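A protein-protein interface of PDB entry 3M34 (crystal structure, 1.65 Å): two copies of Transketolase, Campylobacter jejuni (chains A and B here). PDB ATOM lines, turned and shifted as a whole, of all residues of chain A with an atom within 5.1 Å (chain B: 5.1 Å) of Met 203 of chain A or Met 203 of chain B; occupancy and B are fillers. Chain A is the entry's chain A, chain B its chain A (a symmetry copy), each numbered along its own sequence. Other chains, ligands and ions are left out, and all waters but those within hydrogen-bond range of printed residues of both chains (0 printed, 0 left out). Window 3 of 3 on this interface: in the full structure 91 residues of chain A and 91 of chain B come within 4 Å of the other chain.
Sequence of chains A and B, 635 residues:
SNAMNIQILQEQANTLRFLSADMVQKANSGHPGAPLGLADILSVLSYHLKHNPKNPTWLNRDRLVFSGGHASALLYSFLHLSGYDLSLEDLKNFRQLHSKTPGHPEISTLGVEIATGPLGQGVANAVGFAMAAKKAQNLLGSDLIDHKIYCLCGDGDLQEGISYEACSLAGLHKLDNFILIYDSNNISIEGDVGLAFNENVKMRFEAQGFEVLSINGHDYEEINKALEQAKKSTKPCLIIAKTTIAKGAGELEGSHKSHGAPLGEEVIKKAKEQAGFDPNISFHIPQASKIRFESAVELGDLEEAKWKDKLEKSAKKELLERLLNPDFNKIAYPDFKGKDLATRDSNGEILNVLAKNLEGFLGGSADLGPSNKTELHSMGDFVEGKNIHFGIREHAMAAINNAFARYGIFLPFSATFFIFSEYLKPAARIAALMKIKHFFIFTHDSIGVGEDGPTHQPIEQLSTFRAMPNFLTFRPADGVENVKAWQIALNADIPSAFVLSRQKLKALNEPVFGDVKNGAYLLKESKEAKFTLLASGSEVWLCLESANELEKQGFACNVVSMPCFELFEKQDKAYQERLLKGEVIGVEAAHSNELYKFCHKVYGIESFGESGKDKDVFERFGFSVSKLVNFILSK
N of Asn 200 of chain A is in hydrogen-bond range of O of Ala 207 of chain B (3.0 Å). The backbone NH of Ala 207 of chain B lies within hydrogen-bond range of the side-chain sulfur of Met 203 of chain A (3.6 Å). The backbone carbonyl oxygen of Ala 207 of chain A sits at hydrogen-bond distance from the backbone NH of Asn 200 of chain B (3.0 Å). The backbone NH (N) of Ala 207 of chain A is in hydrogen-bond range of the side-chain sulfur (SD) of Met 203 of chain B (3.6 Å).
OD1 of Asn 200 of chain A lies close to N of Lys 202 of chain A, 3.2 Å away. The side-chain amide oxygen of Asn 200 of chain A is in hydrogen-bond range of the backbone NH of Met 203 of chain A, at 3.0 Å. OE1 of Glu 206 of chain A is in salt-bridge range of NZ of Lys 202 of chain A, at 2.5 Å. The side-chain amide oxygen (OD1) of Asn 200 of chain B sits close to the backbone NH (N) of Lys 202 of chain B (3.2 Å). The side-chain amide oxygen (OD1) of Asn 200 of chain B sits at hydrogen-bond distance from the backbone NH (N) of Met 203 of chain B (3.0 Å). The side-chain carboxylate of Glu 206 of chain B lies within salt-bridge range of the side-chain amino group of Lys 202 of chain B.
Among the printed residues, merely in contact across the chains: Ala 207 of chain A with Arg 204 of chain B (3.4 Å), Arg 204 of chain A with Ala 207 of chain B (3.4 Å), Met 203 of chain A with Met 203 of chain B (3.5 Å), Met 203 of chain A with Glu 206 of chain B (3.98 Å) and Glu 206 of chain A with Met 203 of chain B (3.98 Å).
Of the printed residues of chain B, Asn 200 of chain A touches Ala 207. Of chain B, only Met 203 (3.5 Å), Glu 206 (3.98 Å) and Ala 207 (3.6 Å) come within 4 Å of Met 203 of chain A. Of the printed residues of chain B, Arg 204 of chain A touches Ala 207. Of the printed residues of chain B, Glu 206 of chain A touches Met 203. Printed residues of chain A within 4 Å of Met 203 of chain B: Met 203, Glu 206 and Ala 207. Phe 205 of chain B touches none of the printed residues of chain A. Of the printed residues of chain A, Ala 207 of chain B touches Asn 200, Met 203 and Arg 204. The nearest printed residue of chain A that does not touch Met 203 of chain B is Arg 204 of chain A (5.2 Å). The nearest printed residue of chain A that does not touch Ala 207 of chain B is Val 201 of chain A (5.6 Å).
Of the 8 printed residues of chain A, 5 touch a printed residue of chain B. Hydrophobic or aromatic side chains of chain A within 4 Å of the printed part of chain B: Met 203 and Ala 207. Printed residues of chain B that touch a printed residue of chain A: Asn 200, Met 203, Arg 204, Glu 206 and Ala 207. Hydrophobic or aromatic side chains of chain B that line the printed part of chain A: Met 203 and Ala 207. Along chain B the printed residues that touch a printed residue of chain A span positions 200 to 207.
Met 203 of chain A touches its own counterpart, Met 203 of chain B. Met 203 of chain A touches Glu 206 of chain B, and with the chains exchanged Glu 206 of chain A touches Met 203 of chain B. Met 203 of chain A touches Ala 207 of chain B, and with the chains exchanged Ala 207 of chain A touches Met 203 of chain B. Arg 204 of chain A touches Ala 207 of chain B, and with the chains exchanged Ala 207 of chain A touches Arg 204 of chain B. Of the 9 pairs that touch across the chains among the printed residues, 9 have their exchanged pair printed and touching as well.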
ATOM      1  N   ASN A 200      -5.294  17.157 -18.590  1.00  0.00           N
ATOM      2  CA  ASN A 200      -6.019  17.471 -19.783  1.00  0.00           C
ATOM      3  C   ASN A 200      -6.021  18.988 -19.924  1.00  0.00           C
ATOM      4  O   ASN A 200      -6.788  19.717 -19.304  1.00  0.00           O
ATOM      5  CB  ASN A 200      -7.413  16.906 -19.713  1.00  0.00           C
ATOM      6  CG  ASN A 200      -8.188  17.136 -20.984  1.00  0.00           C
ATOM      7  OD1 ASN A 200      -7.981  18.126 -21.663  1.00  0.00           O
ATOM      8  ND2 ASN A 200      -9.119  16.232 -21.287  1.00  0.00           N
ATOM      9  N   VAL A 201      -5.068  19.477 -20.706  1.00  0.00           N
ATOM     10  CA  VAL A 201      -4.787  20.901 -20.769  1.00  0.00           C
ATOM     11  C   VAL A 201      -5.943  21.653 -21.413  1.00  0.00           C
ATOM     12  O   VAL A 201      -6.292  22.738 -21.012  1.00  0.00           O
ATOM     13  CB  VAL A 201      -3.457  21.115 -21.526  1.00  0.00           C
ATOM     14  CG1 VAL A 201      -3.263  22.634 -21.816  1.00  0.00           C
ATOM     15  CG2 VAL A 201      -2.307  20.488 -20.749  1.00  0.00           C
ATOM     16  N   LYS A 202      -6.649  21.006 -22.361  1.00  0.00           N
ATOM     17  CA  LYS A 202      -7.784  21.643 -23.002  1.00  0.00           C
ATOM     18  C   LYS A 202      -8.912  21.836 -21.972  1.00  0.00           C
ATOM     19  O   LYS A 202      -9.487  22.900 -21.889  1.00  0.00           O
ATOM     20  CB  LYS A 202      -8.263  20.797 -24.179  1.00  0.00           C
ATOM     21  CG  LYS A 202      -9.516  21.301 -24.865  1.00  0.00           C
ATOM     22  CD  LYS A 202      -9.819  20.405 -26.100  1.00  0.00           C
ATOM     23  CE  LYS A 202     -10.745  21.081 -27.102  1.00  0.00           C
ATOM     24  NZ  LYS A 202     -12.146  21.206 -26.655  1.00  0.00           N
ATOM     25  N   MET A 203      -9.144  20.814 -21.154  1.00  0.00           N
ATOM     26  CA  MET A 203     -10.192  20.885 -20.151  1.00  0.00           C
ATOM     27  C   MET A 203      -9.807  21.915 -19.071  1.00  0.00           C
ATOM     28  O   MET A 203     -10.654  22.675 -18.596  1.00  0.00           O
ATOM     29  CB  MET A 203     -10.441  19.489 -19.540  1.00  0.00           C
ATOM     30  CG  MET A 203     -11.616  19.424 -18.652  1.00  0.00           C
ATOM     31  SD  MET A 203     -11.939  17.704 -17.941  1.00  0.00           S
ATOM     32  CE  MET A 203     -11.857  16.817 -19.587  1.00  0.00           C
ATOM     33  N   ARG A 204      -8.535  21.909 -18.669  1.00  0.00           N
ATOM     34  CA  ARG A 204      -8.056  22.918 -17.723  1.00  0.00           C
ATOM     35  C   ARG A 204      -8.383  24.333 -18.144  1.00  0.00           C
ATOM     36  O   ARG A 204      -8.891  25.129 -17.370  1.00  0.00           O
ATOM     37  CB  ARG A 204      -6.568  22.785 -17.495  1.00  0.00           C
ATOM     38  CG  ARG A 204      -5.841  24.063 -17.054  1.00  0.00           C
ATOM     39  CD  ARG A 204      -4.404  23.798 -16.973  1.00  0.00           C
ATOM     40  NE  ARG A 204      -3.616  24.988 -16.726  1.00  0.00           N
ATOM     41  CZ  ARG A 204      -2.275  24.992 -16.593  1.00  0.00           C
ATOM     42  NH1 ARG A 204      -1.570  23.886 -16.577  1.00  0.00           N
ATOM     43  NH2 ARG A 204      -1.666  26.163 -16.410  1.00  0.00           N
ATOM     44  N   PHE A 205      -8.061  24.681 -19.377  1.00  0.00           N
ATOM     45  CA  PHE A 205      -8.259  26.012 -19.857  1.00  0.00           C
ATOM     46  C   PHE A 205      -9.712  26.369 -20.179  1.00  0.00           C
ATOM     47  O   PHE A 205     -10.132  27.492 -19.982  1.00  0.00           O
ATOM     48  CB  PHE A 205      -7.350  26.260 -21.064  1.00  0.00           C
ATOM     49  CG  PHE A 205      -5.946  26.694 -20.670  1.00  0.00           C
ATOM     50  CD1 PHE A 205      -5.005  25.741 -20.358  1.00  0.00           C
ATOM     51  CD2 PHE A 205      -5.614  28.038 -20.657  1.00  0.00           C
ATOM     52  CE1 PHE A 205      -3.685  26.075 -20.012  1.00  0.00           C
ATOM     53  CE2 PHE A 205      -4.285  28.405 -20.342  1.00  0.00           C
ATOM     54  CZ  PHE A 205      -3.352  27.413 -19.991  1.00  0.00           C
ATOM     55  N   GLU A 206     -10.478  25.367 -20.596  1.00  0.00           N
ATOM     56  CA  GLU A 206     -11.878  25.575 -20.796  1.00  0.00           C
ATOM     57  C   GLU A 206     -12.551  25.901 -19.450  1.00  0.00           C
ATOM     58  O   GLU A 206     -13.387  26.763 -19.364  1.00  0.00           O
ATOM     59  CB  GLU A 206     -12.496  24.361 -21.500  1.00  0.00           C
ATOM     60  CG  GLU A 206     -12.182  24.357 -23.008  1.00  0.00           C
ATOM     61  CD  GLU A 206     -12.627  23.095 -23.780  1.00  0.00           C
ATOM     62  OE1 GLU A 206     -12.577  23.105 -25.051  1.00  0.00           O
ATOM     63  OE2 GLU A 206     -13.024  22.092 -23.161  1.00  0.00           O
ATOM     64  N   ALA A 207     -12.103  25.222 -18.392  1.00  0.00           N
ATOM     65  CA  ALA A 207     -12.581  25.509 -17.026  1.00  0.00           C
ATOM     66  C   ALA A 207     -12.328  26.981 -16.597  1.00  0.00           C
ATOM     67  O   ALA A 207     -13.046  27.517 -15.767  1.00  0.00           O
ATOM     68  CB  ALA A 207     -11.970  24.517 -16.033  1.00  0.00           C
ATOM     69  N   ASN B 200     -14.954  27.052 -13.468  1.00  0.00           N
ATOM     70  CA  ASN B 200     -15.688  25.837 -13.289  1.00  0.00           C
ATOM     71  C   ASN B 200     -14.790  24.874 -12.525  1.00  0.00           C
ATOM     72  O   ASN B 200     -13.901  24.220 -13.061  1.00  0.00           O
ATOM     73  CB  ASN B 200     -16.113  25.282 -14.623  1.00  0.00           C
ATOM     74  CG  ASN B 200     -16.966  24.048 -14.483  1.00  0.00           C
ATOM     75  OD1 ASN B 200     -16.802  23.286 -13.546  1.00  0.00           O
ATOM     76  ND2 ASN B 200     -17.859  23.827 -15.447  1.00  0.00           N
ATOM     77  N   VAL B 201     -14.979  24.855 -11.213  1.00  0.00           N
ATOM     78  CA  VAL B 201     -14.063  24.169 -10.318  1.00  0.00           C
ATOM     79  C   VAL B 201     -14.130  22.663 -10.524  1.00  0.00           C
ATOM     80  O   VAL B 201     -13.139  21.974 -10.479  1.00  0.00           O
ATOM     81  CB  VAL B 201     -14.388  24.575  -8.863  1.00  0.00           C
ATOM     82  CG1 VAL B 201     -13.585  23.671  -7.880  1.00  0.00           C
ATOM     83  CG2 VAL B 201     -14.138  26.065  -8.668  1.00  0.00           C
ATOM     84  N   LYS B 202     -15.318  22.143 -10.891  1.00  0.00           N
ATOM     85  CA  LYS B 202     -15.458  20.720 -11.136  1.00  0.00           C
ATOM     86  C   LYS B 202     -14.645  20.332 -12.385  1.00  0.00           C
ATOM     87  O   LYS B 202     -13.922  19.360 -12.365  1.00  0.00           O
ATOM     88  CB  LYS B 202     -16.932  20.362 -11.316  1.00  0.00           C
ATOM     89  CG  LYS B 202     -17.202  18.919 -11.688  1.00  0.00           C
ATOM     90  CD  LYS B 202     -18.738  18.681 -11.731  1.00  0.00           C
ATOM     91  CE  LYS B 202     -19.107  17.207 -11.629  1.00  0.00           C
ATOM     92  NZ  LYS B 202     -18.794  16.411 -12.831  1.00  0.00           N
ATOM     93  N   MET B 203     -14.728  21.160 -13.422  1.00  0.00           N
ATOM     94  CA  MET B 203     -14.011  20.885 -14.655  1.00  0.00           C
ATOM     95  C   MET B 203     -12.496  21.027 -14.414  1.00  0.00           C
ATOM     96  O   MET B 203     -11.699  20.235 -14.926  1.00  0.00           O
ATOM     97  CB  MET B 203     -14.497  21.827 -15.777  1.00  0.00           C
ATOM     98  CG  MET B 203     -13.965  21.497 -17.111  1.00  0.00           C
ATOM     99  SD  MET B 203     -14.597  22.628 -18.486  1.00  0.00           S
ATOM    100  CE  MET B 203     -16.406  22.451 -18.039  1.00  0.00           C
ATOM    101  N   ARG B 204     -12.105  22.058 -13.663  1.00  0.00           N
ATOM    102  CA  ARG B 204     -10.697  22.212 -13.296  1.00  0.00           C
ATOM    103  C   ARG B 204     -10.098  20.965 -12.686  1.00  0.00           C
ATOM    104  O   ARG B 204      -9.031  20.513 -13.072  1.00  0.00           O
ATOM    105  CB  ARG B 204     -10.505  23.382 -12.357  1.00  0.00           C
ATOM    106  CG  ARG B 204      -9.276  23.309 -11.440  1.00  0.00           C
ATOM    107  CD  ARG B 204      -9.286  24.454 -10.529  1.00  0.00           C
ATOM    108  NE  ARG B 204      -8.255  24.385  -9.513  1.00  0.00           N
ATOM    109  CZ  ARG B 204      -8.055  25.331  -8.575  1.00  0.00           C
ATOM    110  NH1 ARG B 204      -8.723  26.459  -8.565  1.00  0.00           N
ATOM    111  NH2 ARG B 204      -7.098  25.126  -7.670  1.00  0.00           N
ATOM    112  N   PHE B 205     -10.764  20.405 -11.693  1.00  0.00           N
ATOM    113  CA  PHE B 205     -10.255  19.265 -10.997  1.00  0.00           C
ATOM    114  C   PHE B 205     -10.366  17.944 -11.762  1.00  0.00           C
ATOM    115  O   PHE B 205      -9.508  17.092 -11.653  1.00  0.00           O
ATOM    116  CB  PHE B 205     -10.924  19.165  -9.623  1.00  0.00           C
ATOM    117  CG  PHE B 205     -10.240  20.019  -8.566  1.00  0.00           C
ATOM    118  CD1 PHE B 205     -10.569  21.350  -8.453  1.00  0.00           C
ATOM    119  CD2 PHE B 205      -9.316  19.449  -7.707  1.00  0.00           C
ATOM    120  CE1 PHE B 205      -9.992  22.185  -7.482  1.00  0.00           C
ATOM    121  CE2 PHE B 205      -8.740  20.256  -6.698  1.00  0.00           C
ATOM    122  CZ  PHE B 205      -9.066  21.623  -6.628  1.00  0.00           C
ATOM    123  N   GLU B 206     -11.397  17.839 -12.593  1.00  0.00           N
ATOM    124  CA  GLU B 206     -11.511  16.696 -13.445  1.00  0.00           C
ATOM    125  C   GLU B 206     -10.342  16.677 -14.445  1.00  0.00           C
ATOM    126  O   GLU B 206      -9.768  15.653 -14.714  1.00  0.00           O
ATOM    127  CB  GLU B 206     -12.885  16.682 -14.125  1.00  0.00           C
ATOM    128  CG  GLU B 206     -13.990  16.199 -13.166  1.00  0.00           C
ATOM    129  CD  GLU B 206     -15.434  16.297 -13.707  1.00  0.00           C
ATOM    130  OE1 GLU B 206     -16.372  15.739 -13.053  1.00  0.00           O
ATOM    131  OE2 GLU B 206     -15.666  16.912 -14.762  1.00  0.00           O
ATOM    132  N   ALA B 207      -9.968  17.862 -14.933  1.00  0.00           N
ATOM    133  CA  ALA B 207      -8.795  18.004 -15.816  1.00  0.00           C
ATOM    134  C   ALA B 207      -7.482  17.498 -15.157  1.00  0.00           C
ATOM    135  O   ALA B 207      -6.561  17.087 -15.846  1.00  0.00           O
ATOM    136  CB  ALA B 207      -8.666  19.452 -16.295  1.00  0.00           C
